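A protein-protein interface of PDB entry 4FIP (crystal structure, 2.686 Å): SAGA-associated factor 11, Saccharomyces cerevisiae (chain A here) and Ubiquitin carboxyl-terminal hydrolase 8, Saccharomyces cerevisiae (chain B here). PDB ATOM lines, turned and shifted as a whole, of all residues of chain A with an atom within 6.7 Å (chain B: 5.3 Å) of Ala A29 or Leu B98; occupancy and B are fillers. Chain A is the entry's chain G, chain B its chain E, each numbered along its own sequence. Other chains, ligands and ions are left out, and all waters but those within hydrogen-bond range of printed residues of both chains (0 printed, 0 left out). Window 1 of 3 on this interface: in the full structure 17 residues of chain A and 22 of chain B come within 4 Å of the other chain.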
ATOM      1  N   ILE A  24     -26.518   5.539  17.564  1.00  0.00           N
ATOM      2  CA  ILE A  24     -25.249   5.045  18.090  1.00  0.00           C
ATOM      3  C   ILE A  24     -24.383   6.192  18.602  1.00  0.00           C
ATOM      4  O   ILE A  24     -23.827   6.126  19.673  1.00  0.00           O
ATOM      5  CB  ILE A  24     -24.436   4.313  17.026  1.00  0.00           C
ATOM      6  CG1 ILE A  24     -25.176   3.056  16.565  1.00  0.00           C
ATOM      7  CG2 ILE A  24     -23.064   3.949  17.590  1.00  0.00           C
ATOM      8  CD1 ILE A  24     -24.590   2.386  15.332  1.00  0.00           C
ATOM      9  N   GLN A  25     -24.280   7.244  17.808  1.00  0.00           N
ATOM     10  CA  GLN A  25     -23.429   8.383  18.124  1.00  0.00           C
ATOM     11  C   GLN A  25     -23.895   9.132  19.359  1.00  0.00           C
ATOM     12  O   GLN A  25     -23.072   9.630  20.106  1.00  0.00           O
ATOM     13  CB  GLN A  25     -23.384   9.341  16.949  1.00  0.00           C
ATOM     14  CG  GLN A  25     -22.572   8.815  15.787  1.00  0.00           C
ATOM     15  CD  GLN A  25     -22.666   9.716  14.571  1.00  0.00           C
ATOM     16  OE1 GLN A  25     -22.747   9.233  13.443  1.00  0.00           O
ATOM     17  NE2 GLN A  25     -22.644  11.033  14.795  1.00  0.00           N
ATOM     18  N   ASP A  26     -25.213   9.232  19.545  1.00  0.00           N
ATOM     19  CA  ASP A  26     -25.793   9.768  20.767  1.00  0.00           C
ATOM     20  C   ASP A  26     -25.398   8.934  21.983  1.00  0.00           C
ATOM     21  O   ASP A  26     -24.990   9.467  22.998  1.00  0.00           O
ATOM     22  CB  ASP A  26     -27.322   9.796  20.658  1.00  0.00           C
ATOM     23  CG  ASP A  26     -27.982  10.418  21.879  1.00  0.00           C
ATOM     24  OD1 ASP A  26     -27.437  11.405  22.391  1.00  0.00           O
ATOM     25  OD2 ASP A  26     -29.038   9.930  22.355  1.00  0.00           O
ATOM     26  N   ILE A  27     -25.555   7.622  21.883  1.00  0.00           N
ATOM     27  CA  ILE A  27     -25.222   6.713  22.972  1.00  0.00           C
ATOM     28  C   ILE A  27     -23.730   6.804  23.304  1.00  0.00           C
ATOM     29  O   ILE A  27     -23.385   6.946  24.475  1.00  0.00           O
ATOM     30  CB  ILE A  27     -25.626   5.267  22.624  1.00  0.00           C
ATOM     31  CG1 ILE A  27     -27.153   5.167  22.565  1.00  0.00           C
ATOM     32  CG2 ILE A  27     -25.064   4.267  23.624  1.00  0.00           C
ATOM     33  CD1 ILE A  27     -27.676   3.930  21.859  1.00  0.00           C
ATOM     34  N   VAL A  28     -22.860   6.780  22.285  1.00  0.00           N
ATOM     35  CA  VAL A  28     -21.406   6.901  22.488  1.00  0.00           C
ATOM     36  C   VAL A  28     -21.045   8.276  23.102  1.00  0.00           C
ATOM     37  O   VAL A  28     -20.223   8.349  24.004  1.00  0.00           O
ATOM     38  CB  VAL A  28     -20.582   6.648  21.180  1.00  0.00           C
ATOM     39  CG1 VAL A  28     -19.094   6.571  21.478  1.00  0.00           C
ATOM     40  CG2 VAL A  28     -21.017   5.373  20.485  1.00  0.00           C
ATOM     41  N   ALA A  29     -21.658   9.361  22.627  1.00  0.00           N
ATOM     42  CA  ALA A  29     -21.361  10.718  23.143  1.00  0.00           C
ATOM     43  C   ALA A  29     -21.589  10.794  24.640  1.00  0.00           C
ATOM     44  O   ALA A  29     -20.730  11.291  25.386  1.00  0.00           O
ATOM     45  CB  ALA A  29     -22.210  11.761  22.450  1.00  0.00           C
ATOM     46  N   ARG A  30     -22.741  10.289  25.082  1.00  0.00           N
ATOM     47  CA  ARG A  30     -23.068  10.303  26.505  1.00  0.00           C
ATOM     48  C   ARG A  30     -22.180   9.430  27.382  1.00  0.00           C
ATOM     49  O   ARG A  30     -22.010   9.749  28.543  1.00  0.00           O
ATOM     50  CB  ARG A  30     -24.499   9.899  26.733  1.00  0.00           C
ATOM     51  CG  ARG A  30     -25.511  10.905  26.239  1.00  0.00           C
ATOM     52  CD  ARG A  30     -26.793  10.169  25.903  1.00  0.00           C
ATOM     53  NE  ARG A  30     -27.836  10.992  25.302  1.00  0.00           N
ATOM     54  CZ  ARG A  30     -28.860  11.526  25.960  1.00  0.00           C
ATOM     55  NH1 ARG A  30     -28.982  11.380  27.273  1.00  0.00           N
ATOM     56  NH2 ARG A  30     -29.767  12.223  25.292  1.00  0.00           N
ATOM     57  N   GLU A  31     -21.621   8.343  26.858  1.00  0.00           N
ATOM     58  CA  GLU A  31     -20.717   7.509  27.664  1.00  0.00           C
ATOM     59  C   GLU A  31     -19.277   8.052  27.713  1.00  0.00           C
ATOM     60  O   GLU A  31     -18.602   7.955  28.746  1.00  0.00           O
ATOM     61  CB  GLU A  31     -20.716   6.051  27.180  1.00  0.00           C
ATOM     62  CG  GLU A  31     -22.014   5.288  27.445  1.00  0.00           C
ATOM     63  CD  GLU A  31     -22.317   5.058  28.923  1.00  0.00           C
ATOM     64  OE1 GLU A  31     -21.496   5.479  29.777  1.00  0.00           O
ATOM     65  OE2 GLU A  31     -23.383   4.462  29.235  1.00  0.00           O
ATOM     66  N   THR A  32     -18.799   8.606  26.607  1.00  0.00           N
ATOM     67  CA  THR A  32     -17.485   9.198  26.613  1.00  0.00           C
ATOM     68  C   THR A  32     -17.491  10.432  27.511  1.00  0.00           C
ATOM     69  O   THR A  32     -16.639  10.542  28.369  1.00  0.00           O
ATOM     70  CB  THR A  32     -16.959   9.530  25.204  1.00  0.00           C
ATOM     71  OG1 THR A  32     -17.775  10.528  24.596  1.00  0.00           O
ATOM     72  CG2 THR A  32     -16.937   8.280  24.333  1.00  0.00           C
ATOM     73  N   THR A  33     -18.460  11.328  27.372  1.00  0.00           N
ATOM     74  CA  THR A  33     -18.466  12.538  28.184  1.00  0.00           C
ATOM     75  C   THR A  33     -18.559  12.230  29.687  1.00  0.00           C
ATOM     76  O   THR A  33     -17.897  12.884  30.484  1.00  0.00           O
ATOM     77  CB  THR A  33     -19.565  13.532  27.760  1.00  0.00           C
ATOM     78  OG1 THR A  33     -20.866  12.982  28.014  1.00  0.00           O
ATOM     79  CG2 THR A  33     -19.444  13.880  26.279  1.00  0.00           C
ATOM     80  N   GLN A  34     -19.356  11.239  30.080  1.00  0.00           N
ATOM     81  CA  GLN A  34     -19.475  10.850  31.499  1.00  0.00           C
ATOM     82  C   GLN A  34     -18.176  10.338  32.072  1.00  0.00           C
ATOM     83  O   GLN A  34     -17.821  10.684  33.187  1.00  0.00           O
ATOM     84  CB  GLN A  34     -20.458   9.712  31.666  1.00  0.00           C
ATOM     85  CG  GLN A  34     -21.916  10.089  31.800  1.00  0.00           C
ATOM     86  CD  GLN A  34     -22.770   8.843  31.948  1.00  0.00           C
ATOM     87  OE1 GLN A  34     -23.448   8.420  30.998  1.00  0.00           O
ATOM     88  NE2 GLN A  34     -22.710   8.220  33.126  1.00  0.00           N
ATOM     89  N   ARG B  33     -29.989  24.454  24.323  1.00  0.00           N
ATOM     90  CA  ARG B  33     -30.572  23.418  25.120  1.00  0.00           C
ATOM     91  C   ARG B  33     -32.022  23.687  25.367  1.00  0.00           C
ATOM     92  O   ARG B  33     -32.851  22.776  25.356  1.00  0.00           O
ATOM     93  CB  ARG B  33     -29.841  23.328  26.453  1.00  0.00           C
ATOM     94  CG  ARG B  33     -28.500  22.642  26.326  1.00  0.00           C
ATOM     95  CD  ARG B  33     -27.641  22.829  27.555  1.00  0.00           C
ATOM     96  NE  ARG B  33     -26.340  22.227  27.316  1.00  0.00           N
ATOM     97  CZ  ARG B  33     -25.254  22.445  28.045  1.00  0.00           C
ATOM     98  NH1 ARG B  33     -25.269  23.268  29.099  1.00  0.00           N
ATOM     99  NH2 ARG B  33     -24.137  21.828  27.702  1.00  0.00           N
ATOM    100  N   GLY B  91     -19.722  23.160  18.207  1.00  0.00           N
ATOM    101  CA  GLY B  91     -21.083  22.729  17.880  1.00  0.00           C
ATOM    102  C   GLY B  91     -21.747  21.991  19.025  1.00  0.00           C
ATOM    103  O   GLY B  91     -21.077  21.353  19.846  1.00  0.00           O
ATOM    104  N   ILE B  92     -23.069  22.102  19.082  1.00  0.00           N
ATOM    105  CA  ILE B  92     -23.893  21.404  20.074  1.00  0.00           C
ATOM    106  C   ILE B  92     -24.710  20.314  19.380  1.00  0.00           C
ATOM    107  O   ILE B  92     -25.480  20.605  18.473  1.00  0.00           O
ATOM    108  CB  ILE B  92     -24.850  22.388  20.775  1.00  0.00           C
ATOM    109  CG1 ILE B  92     -24.050  23.554  21.369  1.00  0.00           C
ATOM    110  CG2 ILE B  92     -25.668  21.680  21.847  1.00  0.00           C
ATOM    111  CD1 ILE B  92     -24.759  24.276  22.491  1.00  0.00           C
ATOM    112  N   ASN B  93     -24.515  19.068  19.791  1.00  0.00           N
ATOM    113  CA  ASN B  93     -25.261  17.943  19.249  1.00  0.00           C
ATOM    114  C   ASN B  93     -26.726  18.105  19.624  1.00  0.00           C
ATOM    115  O   ASN B  93     -27.033  18.274  20.780  1.00  0.00           O
ATOM    116  CB  ASN B  93     -24.675  16.649  19.812  1.00  0.00           C
ATOM    117  CG  ASN B  93     -25.442  15.405  19.397  1.00  0.00           C
ATOM    118  OD1 ASN B  93     -26.664  15.423  19.296  1.00  0.00           O
ATOM    119  ND2 ASN B  93     -24.717  14.289  19.195  1.00  0.00           N
ATOM    120  N   ASN B  96     -28.620  15.679  22.265  1.00  0.00           N
ATOM    121  CA  ASN B  96     -28.258  15.635  23.682  1.00  0.00           C
ATOM    122  C   ASN B  96     -27.707  16.906  24.293  1.00  0.00           C
ATOM    123  O   ASN B  96     -27.416  16.922  25.455  1.00  0.00           O
ATOM    124  CB  ASN B  96     -27.255  14.494  23.931  1.00  0.00           C
ATOM    125  CG  ASN B  96     -25.979  14.607  23.077  1.00  0.00           C
ATOM    126  OD1 ASN B  96     -25.338  15.664  23.010  1.00  0.00           O
ATOM    127  ND2 ASN B  96     -25.590  13.497  22.444  1.00  0.00           N
ATOM    128  N   GLY B  97     -27.537  17.969  23.535  1.00  0.00           N
ATOM    129  CA  GLY B  97     -27.033  19.222  24.104  1.00  0.00           C
ATOM    130  C   GLY B  97     -25.532  19.297  24.400  1.00  0.00           C
ATOM    131  O   GLY B  97     -25.055  20.334  24.901  1.00  0.00           O
ATOM    132  N   LEU B  98     -24.776  18.226  24.123  1.00  0.00           N
ATOM    133  CA  LEU B  98     -23.336  18.193  24.442  1.00  0.00           C
ATOM    134  C   LEU B  98     -22.486  18.971  23.426  1.00  0.00           C
ATOM    135  O   LEU B  98     -22.806  19.015  22.237  1.00  0.00           O
ATOM    136  CB  LEU B  98     -22.827  16.756  24.554  1.00  0.00           C
ATOM    137  CG  LEU B  98     -23.454  15.906  25.661  1.00  0.00           C
ATOM    138  CD1 LEU B  98     -23.030  14.455  25.461  1.00  0.00           C
ATOM    139  CD2 LEU B  98     -23.039  16.417  27.040  1.00  0.00           C
ATOM    140  N   LEU B  99     -21.400  19.576  23.913  1.00  0.00           N
ATOM    141  CA  LEU B  99     -20.616  20.543  23.149  1.00  0.00           C
ATOM    142  C   LEU B  99     -19.387  19.862  22.571  1.00  0.00           C
ATOM    143  O   LEU B  99     -18.596  19.275  23.312  1.00  0.00           O
ATOM    144  CB  LEU B  99     -20.181  21.719  24.042  1.00  0.00           C
ATOM    145  CG  LEU B  99     -19.302  22.772  23.360  1.00  0.00           C
ATOM    146  CD1 LEU B  99     -20.117  23.562  22.318  1.00  0.00           C
ATOM    147  CD2 LEU B  99     -18.637  23.654  24.402  1.00  0.00           C
ATOM    148  N   PHE B 100     -19.229  19.966  21.256  1.00  0.00           N
ATOM    149  CA  PHE B 100     -18.132  19.331  20.559  1.00  0.00           C
ATOM    150  C   PHE B 100     -17.141  20.371  20.022  1.00  0.00           C
ATOM    151  O   PHE B 100     -17.537  21.393  19.462  1.00  0.00           O
ATOM    152  CB  PHE B 100     -18.700  18.467  19.419  1.00  0.00           C
ATOM    153  CG  PHE B 100     -17.746  17.434  18.899  1.00  0.00           C
ATOM    154  CD1 PHE B 100     -17.575  16.233  19.563  1.00  0.00           C
ATOM    155  CD2 PHE B 100     -17.012  17.660  17.749  1.00  0.00           C
ATOM    156  CE1 PHE B 100     -16.680  15.273  19.094  1.00  0.00           C
ATOM    157  CE2 PHE B 100     -16.114  16.708  17.276  1.00  0.00           C
ATOM    158  CZ  PHE B 100     -15.948  15.516  17.944  1.00  0.00           C
ATOM    159  N   TYR B 107     -15.717  15.851  22.562  1.00  0.00           N
ATOM    160  CA  TYR B 107     -16.742  16.529  23.326  1.00  0.00           C
ATOM    161  C   TYR B 107     -16.120  17.127  24.563  1.00  0.00           C
ATOM    162  O   TYR B 107     -15.377  16.455  25.275  1.00  0.00           O
ATOM    163  CB  TYR B 107     -17.849  15.545  23.756  1.00  0.00           C
ATOM    164  CG  TYR B 107     -18.887  15.310  22.694  1.00  0.00           C
ATOM    165  CD1 TYR B 107     -19.858  16.274  22.415  1.00  0.00           C
ATOM    166  CD2 TYR B 107     -18.897  14.137  21.960  1.00  0.00           C
ATOM    167  CE1 TYR B 107     -20.805  16.069  21.424  1.00  0.00           C
ATOM    168  CE2 TYR B 107     -19.825  13.929  20.969  1.00  0.00           C
ATOM    169  CZ  TYR B 107     -20.776  14.894  20.701  1.00  0.00           C
ATOM    170  OH  TYR B 107     -21.700  14.666  19.701  1.00  0.00           O
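The side-chain amide nitrogen (ND2) of Asn B96 lies within hydrogen-bond range of the side-chain carboxylate (OD1) of Asp A26 (2.8 Å).
OG1 of Thr A33 is in hydrogen-bond range of O of Arg A30 (3.5 Å).
ND2 of Asn B93 sits at hydrogen-bond distance from OH of Tyr B107, at 3.1 Å.
The side-chain amide nitrogen (ND2) of Asn B93 lies close to the side-chain amide nitrogen (ND2) of Asn B96.
The side-chain amide oxygen (OD1) of Asn B96 is in hydrogen-bond range of the backbone NH (N) of Leu B98, 2.8 Å away.
The backbone carbonyl oxygen (O) of Arg A30 lies close to the side-chain amide oxygen (OE1) of Gln A34 (3.1 Å).
The side-chain carboxylate (OD1) of Asp A26 is in salt-bridge range of the guanidinium group (NE) of Arg A30.
Among the printed residues, merely in contact across the chains: Thr A33 with Tyr B107, Ala A29 with Tyr B107, Arg A30 with Asn B96, Thr A33 with Leu B98, Ala A29 with Asn B96 and Ala A29 with Leu B98.
Of chain A, only Ala A29 and Thr A33 come within 4 Å of Leu B98.
Of the printed residues of chain B, Thr A33 touches Leu B98 (3.7 Å) and Tyr B107 (3.4 Å).
Of the printed residues of chain B, Asp A26 touches Asn B96 (2.8 Å).
Of the printed residues of chain A, Tyr B107 touches Ala A29 and Thr A33.
Of the printed residues of chain B, Arg A30 touches Asn B96 (3.6 Å).
Of the printed residues of chain A, Asn B96 touches Asp A26 (2.8 Å), Ala A29 (3.8 Å) and Arg A30 (3.6 Å).
Gln A25 touches none of the printed residues of chain B.
Thr A32 touches none of the printed residues of chain B.
The nearest residue of chain B that does not touch Ala A29 is Asn B93 (4.8 Å).
The nearest residue of chain A that does not touch Leu B98 is Arg A30 (4.2 Å).
Of the 11 printed residues of chain A, 4 touch a printed residue of chain B.
Among the printed residues, no Asp or Glu carboxylate lies within 4 Å of a Lys or Arg side-chain nitrogen of the other chain.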
